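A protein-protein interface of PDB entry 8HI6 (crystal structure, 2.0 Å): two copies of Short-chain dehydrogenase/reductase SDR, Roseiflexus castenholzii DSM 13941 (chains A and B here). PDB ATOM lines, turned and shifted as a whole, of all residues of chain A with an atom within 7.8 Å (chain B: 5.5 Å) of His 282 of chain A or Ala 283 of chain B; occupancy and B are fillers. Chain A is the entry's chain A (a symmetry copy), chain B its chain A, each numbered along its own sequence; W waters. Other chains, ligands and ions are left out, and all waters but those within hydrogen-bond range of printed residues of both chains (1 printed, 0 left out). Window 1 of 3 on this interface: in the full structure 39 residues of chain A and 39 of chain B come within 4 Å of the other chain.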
ATOM      1  N   VAL A 161      16.742   1.235   6.825  1.00  0.00           N
ATOM      2  CA  VAL A 161      16.258   0.159   7.682  1.00  0.00           C
ATOM      3  C   VAL A 161      14.743   0.282   7.756  1.00  0.00           C
ATOM      4  O   VAL A 161      14.219   1.341   8.130  1.00  0.00           O
ATOM      5  CB  VAL A 161      16.883   0.225   9.089  1.00  0.00           C
ATOM      6  CG1 VAL A 161      16.275  -0.852  10.005  1.00  0.00           C
ATOM      7  CG2 VAL A 161      18.398   0.082   9.033  1.00  0.00           C
ATOM      8  N   ASN A 163      11.408  -1.444   9.314  1.00  0.00           N
ATOM      9  CA  ASN A 163      10.890  -2.384  10.301  1.00  0.00           C
ATOM     10  C   ASN A 163       9.401  -2.581  10.082  1.00  0.00           C
ATOM     11  O   ASN A 163       8.653  -1.603   9.943  1.00  0.00           O
ATOM     12  CB  ASN A 163      11.165  -1.884  11.721  1.00  0.00           C
ATOM     13  CG  ASN A 163      12.642  -1.784  12.011  1.00  0.00           C
ATOM     14  OD1 ASN A 163      13.449  -2.493  11.411  1.00  0.00           O
ATOM     15  ND2 ASN A 163      13.014  -0.882  12.910  1.00  0.00           N
ATOM     16  N   SER A 190      12.542   0.955  17.431  1.00  0.00           N
ATOM     17  CA  SER A 190      12.770   1.584  16.132  1.00  0.00           C
ATOM     18  C   SER A 190      12.980   3.083  16.264  1.00  0.00           C
ATOM     19  O   SER A 190      13.801   3.667  15.552  1.00  0.00           O
ATOM     20  CB  SER A 190      11.586   1.341  15.196  1.00  0.00           C
ATOM     21  OG  SER A 190      11.393  -0.030  14.984  1.00  0.00           O
ATOM     22  N   ASP A 191      12.219   3.733  17.138  1.00  0.00           N
ATOM     23  CA  ASP A 191      12.405   5.170  17.292  1.00  0.00           C
ATOM     24  C   ASP A 191      13.750   5.486  17.926  1.00  0.00           C
ATOM     25  O   ASP A 191      14.417   6.440  17.514  1.00  0.00           O
ATOM     26  CB  ASP A 191      11.260   5.788  18.096  1.00  0.00           C
ATOM     27  CG  ASP A 191      11.207   7.307  17.937  1.00  0.00           C
ATOM     28  OD1 ASP A 191      10.852   7.809  16.833  1.00  0.00           O
ATOM     29  OD2 ASP A 191      11.594   8.002  18.907  1.00  0.00           O
ATOM     30  N   ALA A 194      16.399   5.017  15.140  1.00  0.00           N
ATOM     31  CA  ALA A 194      16.456   6.142  14.216  1.00  0.00           C
ATOM     32  C   ALA A 194      17.329   7.254  14.776  1.00  0.00           C
ATOM     33  O   ALA A 194      18.114   7.878  14.045  1.00  0.00           O
ATOM     34  CB  ALA A 194      15.046   6.667  13.937  1.00  0.00           C
ATOM     35  N   ARG A 203      18.742   5.782   7.674  1.00  0.00           N
ATOM     36  CA  ARG A 203      17.401   6.082   8.147  1.00  0.00           C
ATOM     37  C   ARG A 203      16.679   4.808   8.594  1.00  0.00           C
ATOM     38  O   ARG A 203      16.960   3.701   8.116  1.00  0.00           O
ATOM     39  CB  ARG A 203      16.605   6.829   7.075  1.00  0.00           C
ATOM     40  CG  ARG A 203      16.357   6.095   5.761  1.00  0.00           C
ATOM     41  CD  ARG A 203      16.125   7.141   4.650  1.00  0.00           C
ATOM     42  NE  ARG A 203      15.730   6.526   3.384  1.00  0.00           N
ATOM     43  CZ  ARG A 203      16.589   6.098   2.478  1.00  0.00           C
ATOM     44  NH1 ARG A 203      17.896   6.219   2.656  1.00  0.00           N
ATOM     45  NH2 ARG A 203      16.130   5.529   1.369  1.00  0.00           N
ATOM     46  N   VAL A 204      15.761   4.977   9.552  1.00  0.00           N
ATOM     47  CA  VAL A 204      15.044   3.865  10.196  1.00  0.00           C
ATOM     48  C   VAL A 204      13.572   4.250  10.247  1.00  0.00           C
ATOM     49  O   VAL A 204      13.208   5.208  10.941  1.00  0.00           O
ATOM     50  CB  VAL A 204      15.555   3.573  11.614  1.00  0.00           C
ATOM     51  CG1 VAL A 204      14.783   2.387  12.245  1.00  0.00           C
ATOM     52  CG2 VAL A 204      17.061   3.320  11.626  1.00  0.00           C
ATOM     53  N   ASN A 205      12.724   3.508   9.534  1.00  0.00           N
ATOM     54  CA  ASN A 205      11.307   3.804   9.458  1.00  0.00           C
ATOM     55  C   ASN A 205      10.500   2.537   9.738  1.00  0.00           C
ATOM     56  O   ASN A 205      11.008   1.424   9.629  1.00  0.00           O
ATOM     57  CB  ASN A 205      10.970   4.405   8.094  1.00  0.00           C
ATOM     58  CG  ASN A 205      11.612   5.773   7.905  1.00  0.00           C
ATOM     59  OD1 ASN A 205      11.193   6.765   8.524  1.00  0.00           O
ATOM     60  ND2 ASN A 205      12.659   5.830   7.086  1.00  0.00           N
ATOM     61  N   THR A 206       9.239   2.711  10.141  1.00  0.00           N
ATOM     62  CA  THR A 206       8.396   1.590  10.542  1.00  0.00           C
ATOM     63  C   THR A 206       7.126   1.543   9.713  1.00  0.00           C
ATOM     64  O   THR A 206       6.398   2.534   9.625  1.00  0.00           O
ATOM     65  CB  THR A 206       8.022   1.675  12.023  1.00  0.00           C
ATOM     66  OG1 THR A 206       9.218   1.727  12.799  1.00  0.00           O
ATOM     67  CG2 THR A 206       7.209   0.418  12.446  1.00  0.00           C
ATOM     68  N   ILE A 207       6.826   0.378   9.148  1.00  0.00           N
ATOM     69  CA  ILE A 207       5.547   0.170   8.485  1.00  0.00           C
ATOM     70  C   ILE A 207       4.600  -0.509   9.467  1.00  0.00           C
ATOM     71  O   ILE A 207       4.970  -1.508  10.096  1.00  0.00           O
ATOM     72  CB  ILE A 207       5.701  -0.685   7.217  1.00  0.00           C
ATOM     73  CG1 ILE A 207       6.715  -0.038   6.265  1.00  0.00           C
ATOM     74  CG2 ILE A 207       4.341  -0.891   6.584  1.00  0.00           C
ATOM     75  CD1 ILE A 207       6.971  -0.859   5.017  1.00  0.00           C
ATOM     76  N   TYR A 208       3.374   0.009   9.572  1.00  0.00           N
ATOM     77  CA  TYR A 208       2.319  -0.551  10.420  1.00  0.00           C
ATOM     78  C   TYR A 208       1.214  -1.055   9.500  1.00  0.00           C
ATOM     79  O   TYR A 208       0.281  -0.304   9.175  1.00  0.00           O
ATOM     80  CB  TYR A 208       1.748   0.502  11.378  1.00  0.00           C
ATOM     81  CG  TYR A 208       2.689   1.040  12.430  1.00  0.00           C
ATOM     82  CD1 TYR A 208       3.606   2.056  12.126  1.00  0.00           C
ATOM     83  CD2 TYR A 208       2.630   0.575  13.748  1.00  0.00           C
ATOM     84  CE1 TYR A 208       4.451   2.568  13.106  1.00  0.00           C
ATOM     85  CE2 TYR A 208       3.456   1.088  14.734  1.00  0.00           C
ATOM     86  CZ  TYR A 208       4.368   2.079  14.407  1.00  0.00           C
ATOM     87  OH  TYR A 208       5.198   2.577  15.382  1.00  0.00           O
ATOM     88  N   LEU A 271      10.341   3.317   0.714  1.00  0.00           N
ATOM     89  CA  LEU A 271      11.281   3.539   1.810  1.00  0.00           C
ATOM     90  C   LEU A 271      12.675   3.014   1.495  1.00  0.00           C
ATOM     91  O   LEU A 271      13.661   3.503   2.066  1.00  0.00           O
ATOM     92  CB  LEU A 271      10.774   2.871   3.097  1.00  0.00           C
ATOM     93  CG  LEU A 271       9.497   3.476   3.703  1.00  0.00           C
ATOM     94  CD1 LEU A 271       9.038   2.670   4.964  1.00  0.00           C
ATOM     95  CD2 LEU A 271       9.759   4.936   4.041  1.00  0.00           C
ATOM     96  N   ALA A 278      14.584  11.725   2.861  1.00  0.00           N
ATOM     97  CA  ALA A 278      14.359  12.721   3.906  1.00  0.00           C
ATOM     98  C   ALA A 278      13.608  12.181   5.124  1.00  0.00           C
ATOM     99  O   ALA A 278      13.369  12.947   6.065  1.00  0.00           O
ATOM    100  CB  ALA A 278      13.597  13.916   3.322  1.00  0.00           C
ATOM    101  N   PHE A 279      13.232  10.897   5.140  1.00  0.00           N
ATOM    102  CA  PHE A 279      12.411  10.312   6.210  1.00  0.00           C
ATOM    103  C   PHE A 279      13.251   9.473   7.169  1.00  0.00           C
ATOM    104  O   PHE A 279      13.933   8.529   6.740  1.00  0.00           O
ATOM    105  CB  PHE A 279      11.316   9.406   5.638  1.00  0.00           C
ATOM    106  CG  PHE A 279      10.255  10.121   4.858  1.00  0.00           C
ATOM    107  CD1 PHE A 279      10.427  10.381   3.504  1.00  0.00           C
ATOM    108  CD2 PHE A 279       9.068  10.505   5.466  1.00  0.00           C
ATOM    109  CE1 PHE A 279       9.442  11.039   2.766  1.00  0.00           C
ATOM    110  CE2 PHE A 279       8.067  11.170   4.740  1.00  0.00           C
ATOM    111  CZ  PHE A 279       8.254  11.432   3.379  1.00  0.00           C
ATOM    112  N   THR A 280      13.149   9.766   8.468  1.00  0.00           N
ATOM    113  CA  THR A 280      13.577   8.798   9.472  1.00  0.00           C
ATOM    114  C   THR A 280      12.679   8.910  10.698  1.00  0.00           C
ATOM    115  O   THR A 280      12.029   9.933  10.929  1.00  0.00           O
ATOM    116  CB  THR A 280      15.057   8.947   9.857  1.00  0.00           C
ATOM    117  OG1 THR A 280      15.505   7.740  10.480  1.00  0.00           O
ATOM    118  CG2 THR A 280      15.291  10.124  10.835  1.00  0.00           C
ATOM    119  N   GLY A 281      12.640   7.827  11.471  1.00  0.00           N
ATOM    120  CA  GLY A 281      11.784   7.757  12.649  1.00  0.00           C
ATOM    121  C   GLY A 281      10.315   7.926  12.347  1.00  0.00           C
ATOM    122  O   GLY A 281       9.569   8.428  13.188  1.00  0.00           O
ATOM    123  N   HIS A 282       9.879   7.511  11.168  1.00  0.00           N
ATOM    124  CA  HIS A 282       8.570   7.858  10.635  1.00  0.00           C
ATOM    125  C   HIS A 282       7.699   6.610  10.525  1.00  0.00           C
ATOM    126  O   HIS A 282       8.183   5.529  10.177  1.00  0.00           O
ATOM    127  CB  HIS A 282       8.723   8.514   9.259  1.00  0.00           C
ATOM    128  CG  HIS A 282       7.570   9.372   8.840  1.00  0.00           C
ATOM    129  ND1 HIS A 282       6.324   8.861   8.549  1.00  0.00           N
ATOM    130  CD2 HIS A 282       7.498  10.699   8.581  1.00  0.00           C
ATOM    131  CE1 HIS A 282       5.524   9.840   8.171  1.00  0.00           C
ATOM    132  NE2 HIS A 282       6.211  10.968   8.183  1.00  0.00           N
ATOM    133  N   ALA A 283       6.413   6.771  10.806  1.00  0.00           N
ATOM    134  CA  ALA A 283       5.438   5.690  10.752  1.00  0.00           C
ATOM    135  C   ALA A 283       4.732   5.717   9.401  1.00  0.00           C
ATOM    136  O   ALA A 283       4.477   6.792   8.855  1.00  0.00           O
ATOM    137  CB  ALA A 283       4.409   5.844  11.878  1.00  0.00           C
ATOM    138  N   PHE A 284       4.408   4.534   8.875  1.00  0.00           N
ATOM    139  CA  PHE A 284       3.660   4.394   7.623  1.00  0.00           C
ATOM    140  C   PHE A 284       2.543   3.379   7.858  1.00  0.00           C
ATOM    141  O   PHE A 284       2.791   2.167   7.902  1.00  0.00           O
ATOM    142  CB  PHE A 284       4.602   3.980   6.476  1.00  0.00           C
ATOM    143  CG  PHE A 284       5.592   5.066   6.121  1.00  0.00           C
ATOM    144  CD1 PHE A 284       6.767   5.212   6.845  1.00  0.00           C
ATOM    145  CD2 PHE A 284       5.302   5.988   5.132  1.00  0.00           C
ATOM    146  CE1 PHE A 284       7.657   6.245   6.560  1.00  0.00           C
ATOM    147  CE2 PHE A 284       6.182   7.028   4.837  1.00  0.00           C
ATOM    148  CZ  PHE A 284       7.357   7.159   5.553  1.00  0.00           C
ATOM    149  N   GLU A 285       1.309   3.881   8.000  1.00  0.00           N
ATOM    150  CA  GLU A 285       0.162   3.085   8.428  1.00  0.00           C
ATOM    151  C   GLU A 285      -0.638   2.633   7.205  1.00  0.00           C
ATOM    152  O   GLU A 285      -1.429   3.392   6.644  1.00  0.00           O
ATOM    153  CB  GLU A 285      -0.680   3.877   9.424  1.00  0.00           C
ATOM    154  CG  GLU A 285       0.175   4.303  10.632  1.00  0.00           C
ATOM    155  CD  GLU A 285      -0.565   5.125  11.690  1.00  0.00           C
ATOM    156  OE1 GLU A 285      -1.793   5.380  11.549  1.00  0.00           O
ATOM    157  OE2 GLU A 285       0.097   5.497  12.684  1.00  0.00           O
ATOM    158  N   ARG B 170       3.479  23.119  13.849  1.00  0.00           N
ATOM    159  CA  ARG B 170       3.518  22.396  15.112  1.00  0.00           C
ATOM    160  C   ARG B 170       4.730  22.746  15.972  1.00  0.00           C
ATOM    161  O   ARG B 170       4.960  22.083  16.988  1.00  0.00           O
ATOM    162  CB  ARG B 170       3.478  20.876  14.839  1.00  0.00           C
ATOM    163  CG  ARG B 170       2.126  20.416  14.251  1.00  0.00           C
ATOM    164  CD  ARG B 170       2.257  19.224  13.286  1.00  0.00           C
ATOM    165  NE  ARG B 170       2.942  18.087  13.897  1.00  0.00           N
ATOM    166  CZ  ARG B 170       3.275  16.984  13.236  1.00  0.00           C
ATOM    167  NH1 ARG B 170       2.927  16.801  11.969  1.00  0.00           N
ATOM    168  NH2 ARG B 170       4.003  16.057  13.848  1.00  0.00           N
ATOM    169  N   ASN B 205      -4.272  13.068   2.013  1.00  0.00           N
ATOM    170  CA  ASN B 205      -3.072  12.961   2.819  1.00  0.00           C
ATOM    171  C   ASN B 205      -2.364  14.314   2.874  1.00  0.00           C
ATOM    172  O   ASN B 205      -2.590  15.181   2.034  1.00  0.00           O
ATOM    173  CB  ASN B 205      -2.165  11.863   2.264  1.00  0.00           C
ATOM    174  CG  ASN B 205      -2.794  10.484   2.407  1.00  0.00           C
ATOM    175  OD1 ASN B 205      -2.888   9.939   3.520  1.00  0.00           O
ATOM    176  ND2 ASN B 205      -3.266   9.928   1.295  1.00  0.00           N
ATOM    177  N   THR B 206      -1.527  14.508   3.895  1.00  0.00           N
ATOM    178  CA  THR B 206      -0.870  15.790   4.121  1.00  0.00           C
ATOM    179  C   THR B 206       0.639  15.630   4.146  1.00  0.00           C
ATOM    180  O   THR B 206       1.169  14.811   4.900  1.00  0.00           O
ATOM    181  CB  THR B 206      -1.326  16.428   5.434  1.00  0.00           C
ATOM    182  OG1 THR B 206      -2.746  16.570   5.410  1.00  0.00           O
ATOM    183  CG2 THR B 206      -0.687  17.836   5.600  1.00  0.00           C
ATOM    184  N   TYR B 208       4.093  17.423   5.288  1.00  0.00           N
ATOM    185  CA  TYR B 208       4.625  18.437   6.200  1.00  0.00           C
ATOM    186  C   TYR B 208       6.102  18.619   5.871  1.00  0.00           C
ATOM    187  O   TYR B 208       6.959  17.932   6.448  1.00  0.00           O
ATOM    188  CB  TYR B 208       4.476  18.011   7.665  1.00  0.00           C
ATOM    189  CG  TYR B 208       3.065  17.880   8.192  1.00  0.00           C
ATOM    190  CD1 TYR B 208       2.311  16.723   7.952  1.00  0.00           C
ATOM    191  CD2 TYR B 208       2.499  18.889   8.978  1.00  0.00           C
ATOM    192  CE1 TYR B 208       1.022  16.596   8.464  1.00  0.00           C
ATOM    193  CE2 TYR B 208       1.224  18.767   9.505  1.00  0.00           C
ATOM    194  CZ  TYR B 208       0.488  17.622   9.240  1.00  0.00           C
ATOM    195  OH  TYR B 208      -0.782  17.507   9.748  1.00  0.00           O
ATOM    196  N   ARG B 244      17.163  14.588  13.206  1.00  0.00           N
ATOM    197  CA  ARG B 244      17.858  13.374  13.620  1.00  0.00           C
ATOM    198  C   ARG B 244      18.693  12.762  12.505  1.00  0.00           C
ATOM    199  O   ARG B 244      19.686  12.076  12.787  1.00  0.00           O
ATOM    200  CB  ARG B 244      16.847  12.334  14.118  1.00  0.00           C
ATOM    201  CG  ARG B 244      16.304  12.677  15.495  1.00  0.00           C
ATOM    202  CD  ARG B 244      15.432  11.555  16.040  1.00  0.00           C
ATOM    203  NE  ARG B 244      14.149  11.505  15.360  1.00  0.00           N
ATOM    204  CZ  ARG B 244      13.205  10.607  15.606  1.00  0.00           C
ATOM    205  NH1 ARG B 244      13.388   9.632  16.487  1.00  0.00           N
ATOM    206  NH2 ARG B 244      12.051  10.688  14.949  1.00  0.00           N
ATOM    207  N   GLY B 281      -5.772  10.125   5.405  1.00  0.00           N
ATOM    208  CA  GLY B 281      -5.644  10.828   6.677  1.00  0.00           C
ATOM    209  C   GLY B 281      -4.267  10.739   7.287  1.00  0.00           C
ATOM    210  O   GLY B 281      -4.134  10.770   8.511  1.00  0.00           O
ATOM    211  N   HIS B 282      -3.234  10.636   6.464  1.00  0.00           N
ATOM    212  CA  HIS B 282      -1.898  10.265   6.902  1.00  0.00           C
ATOM    213  C   HIS B 282      -0.938  11.435   6.712  1.00  0.00           C
ATOM    214  O   HIS B 282      -1.025  12.172   5.725  1.00  0.00           O
ATOM    215  CB  HIS B 282      -1.407   9.049   6.110  1.00  0.00           C
ATOM    216  CG  HIS B 282      -0.328   8.256   6.781  1.00  0.00           C
ATOM    217  ND1 HIS B 282       0.944   8.744   6.981  1.00  0.00           N
ATOM    218  CD2 HIS B 282      -0.312   6.976   7.222  1.00  0.00           C
ATOM    219  CE1 HIS B 282       1.686   7.815   7.554  1.00  0.00           C
ATOM    220  NE2 HIS B 282       0.948   6.731   7.714  1.00  0.00           N
ATOM    221  N   ALA B 283      -0.015  11.590   7.651  1.00  0.00           N
ATOM    222  CA  ALA B 283       0.983  12.651   7.630  1.00  0.00           C
ATOM    223  C   ALA B 283       2.272  12.117   7.017  1.00  0.00           C
ATOM    224  O   ALA B 283       2.627  10.956   7.230  1.00  0.00           O
ATOM    225  CB  ALA B 283       1.255  13.155   9.052  1.00  0.00           C
ATOM    226  N   PHE B 284       2.975  12.971   6.269  1.00  0.00           N
ATOM    227  CA  PHE B 284       4.271  12.635   5.676  1.00  0.00           C
ATOM    228  C   PHE B 284       5.232  13.785   5.969  1.00  0.00           C
ATOM    229  O   PHE B 284       5.159  14.844   5.332  1.00  0.00           O
ATOM    230  CB  PHE B 284       4.119  12.362   4.167  1.00  0.00           C
ATOM    231  CG  PHE B 284       3.318  11.112   3.884  1.00  0.00           C
ATOM    232  CD1 PHE B 284       1.931  11.150   3.875  1.00  0.00           C
ATOM    233  CD2 PHE B 284       3.950   9.892   3.721  1.00  0.00           C
ATOM    234  CE1 PHE B 284       1.186   9.990   3.670  1.00  0.00           C
ATOM    235  CE2 PHE B 284       3.219   8.723   3.519  1.00  0.00           C
ATOM    236  CZ  PHE B 284       1.837   8.771   3.496  1.00  0.00           C
ATOM    237  N   GLU B 285       6.137  13.569   6.933  1.00  0.00           N
ATOM    238  CA  GLU B 285       6.994  14.617   7.479  1.00  0.00           C
ATOM    239  C   GLU B 285       8.361  14.576   6.794  1.00  0.00           C
ATOM    240  O   GLU B 285       9.219  13.759   7.130  1.00  0.00           O
ATOM    241  CB  GLU B 285       7.090  14.474   8.995  1.00  0.00           C
ATOM    242  CG  GLU B 285       5.687  14.524   9.630  1.00  0.00           C
ATOM    243  CD  GLU B 285       5.661  14.368  11.152  1.00  0.00           C
ATOM    244  OE1 GLU B 285       6.739  14.243  11.795  1.00  0.00           O
ATOM    245  OE2 GLU B 285       4.538  14.397  11.705  1.00  0.00           O
HETATM  246  O   HOH W   1      11.168  12.384   8.863  1.00  0.00           O
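His 282 of chain A touches Ala 283 of chain B, and with the chains exchanged Ala 283 of chain A touches His 282 of chain B. His 282 of chain A touches Phe 284 of chain B, and with the chains exchanged Phe 284 of chain A touches His 282 of chain B. His 282 of chain A touches Glu 285 of chain B, and with the chains exchanged Glu 285 of chain A touches His 282 of chain B. Phe 284 of chain A touches its own counterpart, Phe 284 of chain B. 8 positions are printed for both chains. Of the 10 pairs that touch across the chains among the printed residues, 7 have their exchanged pair printed and touching as well.
Of the 20 printed residues of chain A, 7 touch a printed residue of chain B. Printed residues of chain A that touch a printed residue of chain B: Asp 191, Phe 279, Gly 281, His 282, Ala 283, Phe 284 and Glu 285. Among the printed residues, 10 pairs touch across the chains. Among the printed residues, Asp or Glu carboxylates within 4 Å of a Lys or Arg side-chain nitrogen of the other chain: Asp 191 of chain A with Arg 244 of chain B (3.1 Å).
Water W1 bridges O of Glu 285 of chain B and N of Thr 280 of chain A.
His 282 of chain A touches just these residues of chain B: Ala 283, Phe 284 and Glu 285. Ala 283 of chain B touches just one residue of chain A: His 282. Printed residues of chain B within 4 Å of Phe 279 of chain A: Glu 285. Printed residues of chain A within 4 Å of His 282 of chain B: Ala 283, Phe 284 and Glu 285. Of the printed residues of chain B, Phe 284 of chain A touches His 282 and Phe 284. Of the printed residues of chain A, Phe 284 of chain B touches His 282 (3.6 Å) and Phe 284 (3.7 Å). Of the printed residues of chain A, Arg 244 of chain B touches Asp 191 (3.1 Å) and Gly 281 (3.7 Å). Val 161 of chain A touches none of the printed residues of chain B. Gly 281 of chain B touches none of the printed residues of chain A. The nearest residue of chain B that does not touch His 282 of chain A is His 282 of chain B (4.4 Å). The nearest printed residue of chain B that does not touch Ala 283 of chain A is Ala 283 of chain B (4.8 Å).
O of Glu 285 of chain B touches CD2 of Phe 279 of chain A, at 3.7 Å. Gly 281 of chain A touches Arg 244 of chain B (CA to NH2, 3.7 Å). His 282 of chain A touches Ala 283 of chain B (CE1 to O, 3.2 Å). His 282 of chain A touches Phe 284 of chain B. Ala 283 of chain A touches His 282 of chain B. Phe 284 of chain A touches His 282 of chain B (CA to NE2, 3.6 Å). Phe 284 of chain A touches Phe 284 of chain B.
The guanidinium group (NH1) of Arg 244 of chain B lies within salt-bridge range of the side-chain carboxylate (OD1) of Asp 191 of chain A, 3.1 Å away. A ring nitrogen (NE2) of His 282 of chain B lies within hydrogen-bond range of the backbone NH of Glu 285 of chain A (2.9 Å). The backbone NH (N) of Glu 285 of chain B lies within hydrogen-bond range of a ring nitrogen (NE2) of His 282 of chain A (2.9 Å).
The side-chain carboxylate of Glu 285 of chain B lies within salt-bridge range of the guanidinium group of Arg 170 of chain B (2.8 Å). The backbone NH of Thr 206 of chain B lies within hydrogen-bond range of the backbone carbonyl oxygen of His 282 of chain B (3.0 Å). The backbone carbonyl oxygen (O) of Thr 206 of chain B lies within hydrogen-bond range of the backbone NH (N) of Phe 284 of chain B, at 2.9 Å. The backbone NH (N) of Gly 281 of chain A lies within hydrogen-bond range of the backbone carbonyl oxygen (O) of Val 204 of chain A (2.7 Å). OD1 of Asn 205 of chain A is in hydrogen-bond range of N of Gly 281 of chain A, 3.5 Å away. The side-chain amide oxygen of Asn 205 of chain A sits at hydrogen-bond distance from the backbone NH of His 282 of chain A (3.0 Å).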
